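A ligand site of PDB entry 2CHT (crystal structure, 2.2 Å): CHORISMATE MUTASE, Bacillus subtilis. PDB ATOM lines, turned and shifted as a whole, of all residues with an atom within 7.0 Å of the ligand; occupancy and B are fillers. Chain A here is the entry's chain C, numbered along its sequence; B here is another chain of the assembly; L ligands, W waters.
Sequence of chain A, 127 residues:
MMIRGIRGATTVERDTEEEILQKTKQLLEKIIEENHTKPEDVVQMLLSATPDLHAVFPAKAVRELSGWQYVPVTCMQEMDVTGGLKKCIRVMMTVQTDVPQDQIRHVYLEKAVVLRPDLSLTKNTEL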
ATOM      1  N   LEU A  21     -17.513  -0.468   4.242  1.00  0.00           N
ATOM      2  CA  LEU A  21     -18.663   0.381   3.994  1.00  0.00           C
ATOM      3  C   LEU A  21     -19.794   0.045   4.942  1.00  0.00           C
ATOM      4  O   LEU A  21     -20.473   0.956   5.410  1.00  0.00           O
ATOM      5  CB  LEU A  21     -19.139   0.249   2.538  1.00  0.00           C
ATOM      6  CG  LEU A  21     -18.110   0.526   1.409  1.00  0.00           C
ATOM      7  CD1 LEU A  21     -18.863   0.702   0.115  1.00  0.00           C
ATOM      8  CD2 LEU A  21     -17.301   1.803   1.660  1.00  0.00           C
ATOM      9  N   LEU A  47     -12.306  10.793   8.368  1.00  0.00           N
ATOM     10  CA  LEU A  47     -12.385   9.413   8.734  1.00  0.00           C
ATOM     11  C   LEU A  47     -10.951   8.946   8.613  1.00  0.00           C
ATOM     12  O   LEU A  47     -10.224   9.374   7.702  1.00  0.00           O
ATOM     13  CB  LEU A  47     -13.297   8.672   7.777  1.00  0.00           C
ATOM     14  CG  LEU A  47     -14.782   8.838   8.089  1.00  0.00           C
ATOM     15  CD1 LEU A  47     -15.546   9.176   6.851  1.00  0.00           C
ATOM     16  CD2 LEU A  47     -15.380   7.528   8.527  1.00  0.00           C
ATOM     17  N   VAL A  56     -11.187  -0.120   0.491  1.00  0.00           N
ATOM     18  CA  VAL A  56     -11.971   1.020   0.070  1.00  0.00           C
ATOM     19  C   VAL A  56     -11.764   2.181   1.044  1.00  0.00           C
ATOM     20  O   VAL A  56     -11.251   1.984   2.140  1.00  0.00           O
ATOM     21  CB  VAL A  56     -13.453   0.560  -0.013  1.00  0.00           C
ATOM     22  CG1 VAL A  56     -13.937   0.221   1.377  1.00  0.00           C
ATOM     23  CG2 VAL A  56     -14.321   1.606  -0.674  1.00  0.00           C
ATOM     24  N   PHE A  57     -12.100   3.398   0.583  1.00  0.00           N
ATOM     25  CA  PHE A  57     -12.102   4.614   1.376  1.00  0.00           C
ATOM     26  C   PHE A  57     -13.411   4.573   2.179  1.00  0.00           C
ATOM     27  O   PHE A  57     -14.477   4.480   1.542  1.00  0.00           O
ATOM     28  CB  PHE A  57     -12.108   5.884   0.507  1.00  0.00           C
ATOM     29  CG  PHE A  57     -10.784   6.240  -0.189  1.00  0.00           C
ATOM     30  CD1 PHE A  57      -9.726   6.790   0.552  1.00  0.00           C
ATOM     31  CD2 PHE A  57     -10.643   6.053  -1.562  1.00  0.00           C
ATOM     32  CE1 PHE A  57      -8.552   7.132  -0.105  1.00  0.00           C
ATOM     33  CE2 PHE A  57      -9.470   6.404  -2.199  1.00  0.00           C
ATOM     34  CZ  PHE A  57      -8.412   6.945  -1.479  1.00  0.00           C
ATOM     35  N   PRO A  58     -13.444   4.668   3.524  1.00  0.00           N
ATOM     36  CA  PRO A  58     -14.675   4.619   4.319  1.00  0.00           C
ATOM     37  C   PRO A  58     -15.619   5.791   4.005  1.00  0.00           C
ATOM     38  O   PRO A  58     -16.824   5.693   4.205  1.00  0.00           O
ATOM     39  CB  PRO A  58     -14.160   4.600   5.753  1.00  0.00           C
ATOM     40  CG  PRO A  58     -12.729   4.161   5.665  1.00  0.00           C
ATOM     41  CD  PRO A  58     -12.289   4.863   4.398  1.00  0.00           C
ATOM     42  N   ALA A  59     -15.134   6.927   3.473  1.00  0.00           N
ATOM     43  CA  ALA A  59     -15.970   8.045   3.105  1.00  0.00           C
ATOM     44  C   ALA A  59     -17.055   7.681   2.120  1.00  0.00           C
ATOM     45  O   ALA A  59     -18.135   8.275   2.120  1.00  0.00           O
ATOM     46  CB  ALA A  59     -15.160   9.153   2.478  1.00  0.00           C
ATOM     47  N   LYS A  60     -16.830   6.665   1.302  1.00  0.00           N
ATOM     48  CA  LYS A  60     -17.847   6.211   0.386  1.00  0.00           C
ATOM     49  C   LYS A  60     -19.092   5.745   1.144  1.00  0.00           C
ATOM     50  O   LYS A  60     -20.176   5.842   0.564  1.00  0.00           O
ATOM     51  CB  LYS A  60     -17.210   5.087  -0.467  1.00  0.00           C
ATOM     52  CG  LYS A  60     -18.017   4.525  -1.611  1.00  0.00           C
ATOM     53  CD  LYS A  60     -17.188   3.431  -2.298  1.00  0.00           C
ATOM     54  CE  LYS A  60     -17.950   2.768  -3.455  1.00  0.00           C
ATOM     55  NZ  LYS A  60     -17.159   1.704  -4.037  1.00  0.00           N
ATOM     56  N   ALA A  61     -19.038   5.296   2.419  1.00  0.00           N
ATOM     57  CA  ALA A  61     -20.249   4.882   3.145  1.00  0.00           C
ATOM     58  C   ALA A  61     -21.155   6.063   3.407  1.00  0.00           C
ATOM     59  O   ALA A  61     -22.379   5.945   3.481  1.00  0.00           O
ATOM     60  CB  ALA A  61     -19.945   4.272   4.485  1.00  0.00           C
ATOM     61  N   VAL A  62     -20.585   7.275   3.441  1.00  0.00           N
ATOM     62  CA  VAL A  62     -21.343   8.492   3.713  1.00  0.00           C
ATOM     63  C   VAL A  62     -22.395   8.687   2.638  1.00  0.00           C
ATOM     64  O   VAL A  62     -23.547   9.060   2.909  1.00  0.00           O
ATOM     65  CB  VAL A  62     -20.364   9.695   3.772  1.00  0.00           C
ATOM     66  CG1 VAL A  62     -21.135  10.967   4.157  1.00  0.00           C
ATOM     67  CG2 VAL A  62     -19.299   9.434   4.821  1.00  0.00           C
ATOM     68  N   ARG A  63     -22.026   8.290   1.416  1.00  0.00           N
ATOM     69  CA  ARG A  63     -22.915   8.387   0.280  1.00  0.00           C
ATOM     70  C   ARG A  63     -24.133   7.496   0.438  1.00  0.00           C
ATOM     71  O   ARG A  63     -25.188   7.751  -0.130  1.00  0.00           O
ATOM     72  CB  ARG A  63     -22.133   8.016  -1.002  1.00  0.00           C
ATOM     73  CG  ARG A  63     -21.247   9.169  -1.543  1.00  0.00           C
ATOM     74  CD  ARG A  63     -19.750   9.075  -1.218  1.00  0.00           C
ATOM     75  NE  ARG A  63     -19.097   8.023  -1.995  1.00  0.00           N
ATOM     76  CZ  ARG A  63     -18.213   8.281  -2.947  1.00  0.00           C
ATOM     77  NH1 ARG A  63     -17.847   9.523  -3.259  1.00  0.00           N
ATOM     78  NH2 ARG A  63     -17.667   7.273  -3.637  1.00  0.00           N
ATOM     79  N   VAL A  73     -16.018  15.271   3.180  1.00  0.00           N
ATOM     80  CA  VAL A  73     -15.358  14.200   3.925  1.00  0.00           C
ATOM     81  C   VAL A  73     -13.929  14.047   3.405  1.00  0.00           C
ATOM     82  O   VAL A  73     -13.699  14.389   2.253  1.00  0.00           O
ATOM     83  CB  VAL A  73     -15.904  12.786   3.727  1.00  0.00           C
ATOM     84  CG1 VAL A  73     -15.703  12.057   5.031  1.00  0.00           C
ATOM     85  CG2 VAL A  73     -17.352  12.735   3.460  1.00  0.00           C
ATOM     86  N   THR A  74     -12.936  13.576   4.156  1.00  0.00           N
ATOM     87  CA  THR A  74     -11.671  13.162   3.588  1.00  0.00           C
ATOM     88  C   THR A  74     -11.060  12.218   4.601  1.00  0.00           C
ATOM     89  O   THR A  74     -11.460  12.169   5.783  1.00  0.00           O
ATOM     90  CB  THR A  74     -10.806  14.438   3.253  1.00  0.00           C
ATOM     91  OG1 THR A  74     -10.135  14.020   2.066  1.00  0.00           O
ATOM     92  CG2 THR A  74      -9.767  14.918   4.202  1.00  0.00           C
ATOM     93  N   CYS A  75     -10.134  11.368   4.150  1.00  0.00           N
ATOM     94  CA  CYS A  75      -9.582  10.336   4.997  1.00  0.00           C
ATOM     95  C   CYS A  75      -8.093  10.529   5.253  1.00  0.00           C
ATOM     96  O   CYS A  75      -7.395  11.252   4.545  1.00  0.00           O
ATOM     97  CB  CYS A  75      -9.819   8.962   4.363  1.00  0.00           C
ATOM     98  SG  CYS A  75     -11.519   8.671   3.820  1.00  0.00           S
ATOM     99  N   MET A  76      -7.619   9.903   6.309  1.00  0.00           N
ATOM    100  CA  MET A  76      -6.197   9.919   6.547  1.00  0.00           C
ATOM    101  C   MET A  76      -5.751   8.609   7.178  1.00  0.00           C
ATOM    102  O   MET A  76      -6.549   7.813   7.676  1.00  0.00           O
ATOM    103  CB  MET A  76      -5.823  11.086   7.455  1.00  0.00           C
ATOM    104  CG  MET A  76      -6.232  11.041   8.892  1.00  0.00           C
ATOM    105  SD  MET A  76      -7.914  11.611   9.093  1.00  0.00           S
ATOM    106  CE  MET A  76      -7.497  12.824  10.305  1.00  0.00           C
ATOM    107  N   ARG B   7     -13.718  20.909   0.049  1.00  0.00           N
ATOM    108  CA  ARG B   7     -12.944  19.854  -0.560  1.00  0.00           C
ATOM    109  C   ARG B   7     -12.338  20.173  -1.903  1.00  0.00           C
ATOM    110  O   ARG B   7     -12.973  20.789  -2.756  1.00  0.00           O
ATOM    111  CB  ARG B   7     -13.772  18.589  -0.778  1.00  0.00           C
ATOM    112  CG  ARG B   7     -13.921  17.678   0.437  1.00  0.00           C
ATOM    113  CD  ARG B   7     -12.565  17.359   1.080  1.00  0.00           C
ATOM    114  NE  ARG B   7     -11.510  16.928   0.158  1.00  0.00           N
ATOM    115  CZ  ARG B   7     -11.618  15.856  -0.656  1.00  0.00           C
ATOM    116  NH1 ARG B   7     -12.694  15.063  -0.716  1.00  0.00           N
ATOM    117  NH2 ARG B   7     -10.593  15.612  -1.484  1.00  0.00           N
ATOM    118  N   GLY B   8     -11.113  19.708  -2.076  1.00  0.00           N
ATOM    119  CA  GLY B   8     -10.418  19.827  -3.329  1.00  0.00           C
ATOM    120  C   GLY B   8      -9.520  18.615  -3.534  1.00  0.00           C
ATOM    121  O   GLY B   8      -9.166  17.961  -2.546  1.00  0.00           O
ATOM    122  N   ALA B   9      -9.153  18.288  -4.764  1.00  0.00           N
ATOM    123  CA  ALA B   9      -8.241  17.194  -5.096  1.00  0.00           C
ATOM    124  C   ALA B   9      -7.610  17.500  -6.443  1.00  0.00           C
ATOM    125  O   ALA B   9      -8.270  18.116  -7.296  1.00  0.00           O
ATOM    126  CB  ALA B   9      -8.971  15.883  -5.219  1.00  0.00           C
ATOM    127  N   SER B  48      -3.847  16.396   2.306  1.00  0.00           N
ATOM    128  CA  SER B  48      -3.326  15.030   2.358  1.00  0.00           C
ATOM    129  C   SER B  48      -2.654  14.564   1.060  1.00  0.00           C
ATOM    130  O   SER B  48      -3.218  14.795  -0.019  1.00  0.00           O
ATOM    131  CB  SER B  48      -4.439  14.039   2.637  1.00  0.00           C
ATOM    132  OG  SER B  48      -5.400  14.017   1.585  1.00  0.00           O
ATOM    133  N   GLU B  78      -2.912  10.322   3.078  1.00  0.00           N
ATOM    134  CA  GLU B  78      -4.066   9.590   2.584  1.00  0.00           C
ATOM    135  C   GLU B  78      -3.763   8.111   2.814  1.00  0.00           C
ATOM    136  O   GLU B  78      -2.605   7.675   2.772  1.00  0.00           O
ATOM    137  CB  GLU B  78      -4.240   9.883   1.081  1.00  0.00           C
ATOM    138  CG  GLU B  78      -5.497   9.301   0.447  1.00  0.00           C
ATOM    139  CD  GLU B  78      -6.772  10.018   0.841  1.00  0.00           C
ATOM    140  OE1 GLU B  78      -6.934  11.159   0.441  1.00  0.00           O
ATOM    141  OE2 GLU B  78      -7.612   9.456   1.526  1.00  0.00           O
ATOM    142  N   MET B  79      -4.792   7.326   3.112  1.00  0.00           N
ATOM    143  CA  MET B  79      -4.609   5.911   3.291  1.00  0.00           C
ATOM    144  C   MET B  79      -4.410   5.258   1.938  1.00  0.00           C
ATOM    145  O   MET B  79      -4.982   5.717   0.934  1.00  0.00           O
ATOM    146  CB  MET B  79      -5.819   5.283   3.994  1.00  0.00           C
ATOM    147  CG  MET B  79      -7.146   5.363   3.331  1.00  0.00           C
ATOM    148  SD  MET B  79      -8.494   4.973   4.458  1.00  0.00           S
ATOM    149  CE  MET B  79      -9.027   3.402   3.850  1.00  0.00           C
ATOM    150  N   LEU B  85      -6.470   6.641  -6.573  1.00  0.00           N
ATOM    151  CA  LEU B  85      -5.871   7.547  -7.508  1.00  0.00           C
ATOM    152  C   LEU B  85      -4.437   7.724  -7.046  1.00  0.00           C
ATOM    153  O   LEU B  85      -4.212   8.075  -5.890  1.00  0.00           O
ATOM    154  CB  LEU B  85      -6.679   8.850  -7.463  1.00  0.00           C
ATOM    155  CG  LEU B  85      -6.432  10.078  -8.322  1.00  0.00           C
ATOM    156  CD1 LEU B  85      -5.822   9.765  -9.676  1.00  0.00           C
ATOM    157  CD2 LEU B  85      -7.797  10.694  -8.531  1.00  0.00           C
ATOM    158  N   CYS B  88      -2.028  11.637  -5.923  1.00  0.00           N
ATOM    159  CA  CYS B  88      -3.081  12.594  -5.686  1.00  0.00           C
ATOM    160  C   CYS B  88      -2.955  13.355  -4.363  1.00  0.00           C
ATOM    161  O   CYS B  88      -2.547  12.812  -3.306  1.00  0.00           O
ATOM    162  CB  CYS B  88      -4.355  11.787  -5.822  1.00  0.00           C
ATOM    163  SG  CYS B  88      -5.783  12.756  -5.362  1.00  0.00           S
ATOM    164  N   ARG B  90      -5.128  16.013  -1.852  1.00  0.00           N
ATOM    165  CA  ARG B  90      -6.474  16.429  -1.549  1.00  0.00           C
ATOM    166  C   ARG B  90      -6.485  17.515  -0.476  1.00  0.00           C
ATOM    167  O   ARG B  90      -5.549  17.531   0.332  1.00  0.00           O
ATOM    168  CB  ARG B  90      -7.234  15.200  -1.116  1.00  0.00           C
ATOM    169  CG  ARG B  90      -7.480  14.367  -2.358  1.00  0.00           C
ATOM    170  CD  ARG B  90      -8.027  12.974  -2.139  1.00  0.00           C
ATOM    171  NE  ARG B  90      -7.043  12.025  -2.638  1.00  0.00           N
ATOM    172  CZ  ARG B  90      -7.362  10.800  -3.021  1.00  0.00           C
ATOM    173  NH1 ARG B  90      -8.610  10.336  -2.999  1.00  0.00           N
ATOM    174  NH2 ARG B  90      -6.384   9.987  -3.407  1.00  0.00           N
ATOM    175  N   TYR B 108     -12.070  19.741  -8.319  1.00  0.00           N
ATOM    176  CA  TYR B 108     -11.288  18.562  -8.670  1.00  0.00           C
ATOM    177  C   TYR B 108     -10.538  18.853  -9.961  1.00  0.00           C
ATOM    178  O   TYR B 108     -11.158  19.126 -10.979  1.00  0.00           O
ATOM    179  CB  TYR B 108     -12.237  17.399  -8.795  1.00  0.00           C
ATOM    180  CG  TYR B 108     -12.783  17.029  -7.414  1.00  0.00           C
ATOM    181  CD1 TYR B 108     -12.084  16.126  -6.594  1.00  0.00           C
ATOM    182  CD2 TYR B 108     -13.954  17.625  -6.924  1.00  0.00           C
ATOM    183  CE1 TYR B 108     -12.532  15.828  -5.318  1.00  0.00           C
ATOM    184  CE2 TYR B 108     -14.409  17.324  -5.637  1.00  0.00           C
ATOM    185  CZ  TYR B 108     -13.698  16.437  -4.849  1.00  0.00           C
ATOM    186  OH  TYR B 108     -14.132  16.192  -3.575  1.00  0.00           O
ATOM    187  N   ALA B 112      -7.824  14.205 -11.174  1.00  0.00           N
ATOM    188  CA  ALA B 112      -8.709  14.080 -10.024  1.00  0.00           C
ATOM    189  C   ALA B 112     -10.156  14.442 -10.310  1.00  0.00           C
ATOM    190  O   ALA B 112     -11.052  14.259  -9.479  1.00  0.00           O
ATOM    191  CB  ALA B 112      -8.260  14.941  -8.896  1.00  0.00           C
ATOM    192  N   LEU B 115     -12.782  11.833  -9.393  1.00  0.00           N
ATOM    193  CA  LEU B 115     -13.132  11.488  -8.023  1.00  0.00           C
ATOM    194  C   LEU B 115     -14.563  11.898  -7.667  1.00  0.00           C
ATOM    195  O   LEU B 115     -15.171  11.253  -6.810  1.00  0.00           O
ATOM    196  CB  LEU B 115     -12.201  12.156  -7.047  1.00  0.00           C
ATOM    197  CG  LEU B 115     -10.803  11.579  -6.874  1.00  0.00           C
ATOM    198  CD1 LEU B 115     -10.077  12.475  -5.894  1.00  0.00           C
ATOM    199  CD2 LEU B 115     -10.854  10.126  -6.393  1.00  0.00           C
HETATM  200  C1  LIG L   1     -13.858   9.919  -1.243  1.00  0.00           C
HETATM  201  C2  LIG L   1     -13.842  11.075  -0.257  1.00  0.00           C
HETATM  202  C3  LIG L   1     -12.708  11.563   0.289  1.00  0.00           C
HETATM  203  C4  LIG L   1     -11.334  11.184  -0.208  1.00  0.00           C
HETATM  204  O1  LIG L   1     -10.588  10.848   0.928  1.00  0.00           O
HETATM  205  C5  LIG L   1     -11.374  10.072  -1.289  1.00  0.00           C
HETATM  206  C6  LIG L   1     -12.548   9.132  -1.049  1.00  0.00           C
HETATM  207  O2  LIG L   1     -11.450  10.509  -2.646  1.00  0.00           O
HETATM  208  C7  LIG L   1     -12.629  11.098  -3.202  1.00  0.00           C
HETATM  209  C8  LIG L   1     -13.914  10.396  -2.709  1.00  0.00           C
HETATM  210  C9  LIG L   1     -15.083   9.026  -0.982  1.00  0.00           C
HETATM  211  O3  LIG L   1     -16.188   9.545  -0.878  1.00  0.00           O
HETATM  212  O4  LIG L   1     -14.948   7.803  -0.866  1.00  0.00           O
HETATM  213  C10 LIG L   1     -12.582  12.636  -3.036  1.00  0.00           C
HETATM  214  O5  LIG L   1     -11.490  13.187  -2.790  1.00  0.00           O
HETATM  215  O6  LIG L   1     -13.637  13.297  -3.161  1.00  0.00           O
HETATM  216  O   HOH W   1     -14.174   6.476  -3.333  1.00  0.00           O
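NE of Arg 90 of chain B lies within salt-bridge range of OE1 of Glu 78 of chain B, 3.2 Å away.
The backbone NH (N) of Ser 48 of chain B is in hydrogen-bond range of the backbone carbonyl oxygen (O) of Arg 90 of chain B, 2.8 Å away.
The side-chain sulfur of Cys 88 of chain B is in hydrogen-bond range of the guanidinium group of Arg 90 of chain B (3.1 Å).
The guanidinium group (NH1) of Arg 7 of chain B lies within hydrogen-bond range of the side-chain hydroxyl (OH) of Tyr 108 of chain B (3.4 Å).
The guanidinium group (NH1) of Arg 7 of chain B sits at hydrogen-bond distance from the backbone carbonyl oxygen (O) of Val 73 (3.2 Å).
The side-chain carboxylate (OE1) of Glu 78 of chain B lies within hydrogen-bond range of the side-chain hydroxyl (OG) of Ser 48 of chain B (3.4 Å).
O of Thr 74 lies within hydrogen-bond range of N of Leu 47 (3.0 Å).
Phe 57 touches the ligand.
CB of Ala 59 touches C9 of the ligand (3.5 Å).
Val 73 touches the ligand.
Leu 115 of chain B touches the ligand.
Hydrophobic or aromatic side chains within 4 Å of the ligand: Phe 57, Ala 59, Tyr 108 of chain B and Leu 115 of chain B.
NH1 of Arg 90 of chain B lies within hydrogen-bond range of O2 of the ligand (2.9 Å).
An oxygen (O5) of the ligand lies within salt-bridge range of the guanidinium group (NH2) of Arg 7 of chain B (2.9 Å).
The guanidinium group of Arg 63 is in salt-bridge range of an oxygen (O3) of the ligand (2.9 Å).
OH of Tyr 108 of chain B lies within hydrogen-bond range of O6 of the ligand, at 3.0 Å.
The backbone NH (N) of Lys 60 sits at hydrogen-bond distance from an oxygen (O4) of the ligand.
The backbone NH (N) of Cys 75 is in hydrogen-bond range of an oxygen (O1) of the ligand (3.3 Å).
An oxygen (O1) of the ligand sits at hydrogen-bond distance from the side-chain sulfur of Cys 75 (3.7 Å).
OE2 of Glu 78 of chain B lies within hydrogen-bond range of O1 of the ligand (3.3 Å).
An oxygen (O1) of the ligand sits at hydrogen-bond distance from the side-chain hydroxyl (OG1) of Thr 74, at 3.4 Å.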
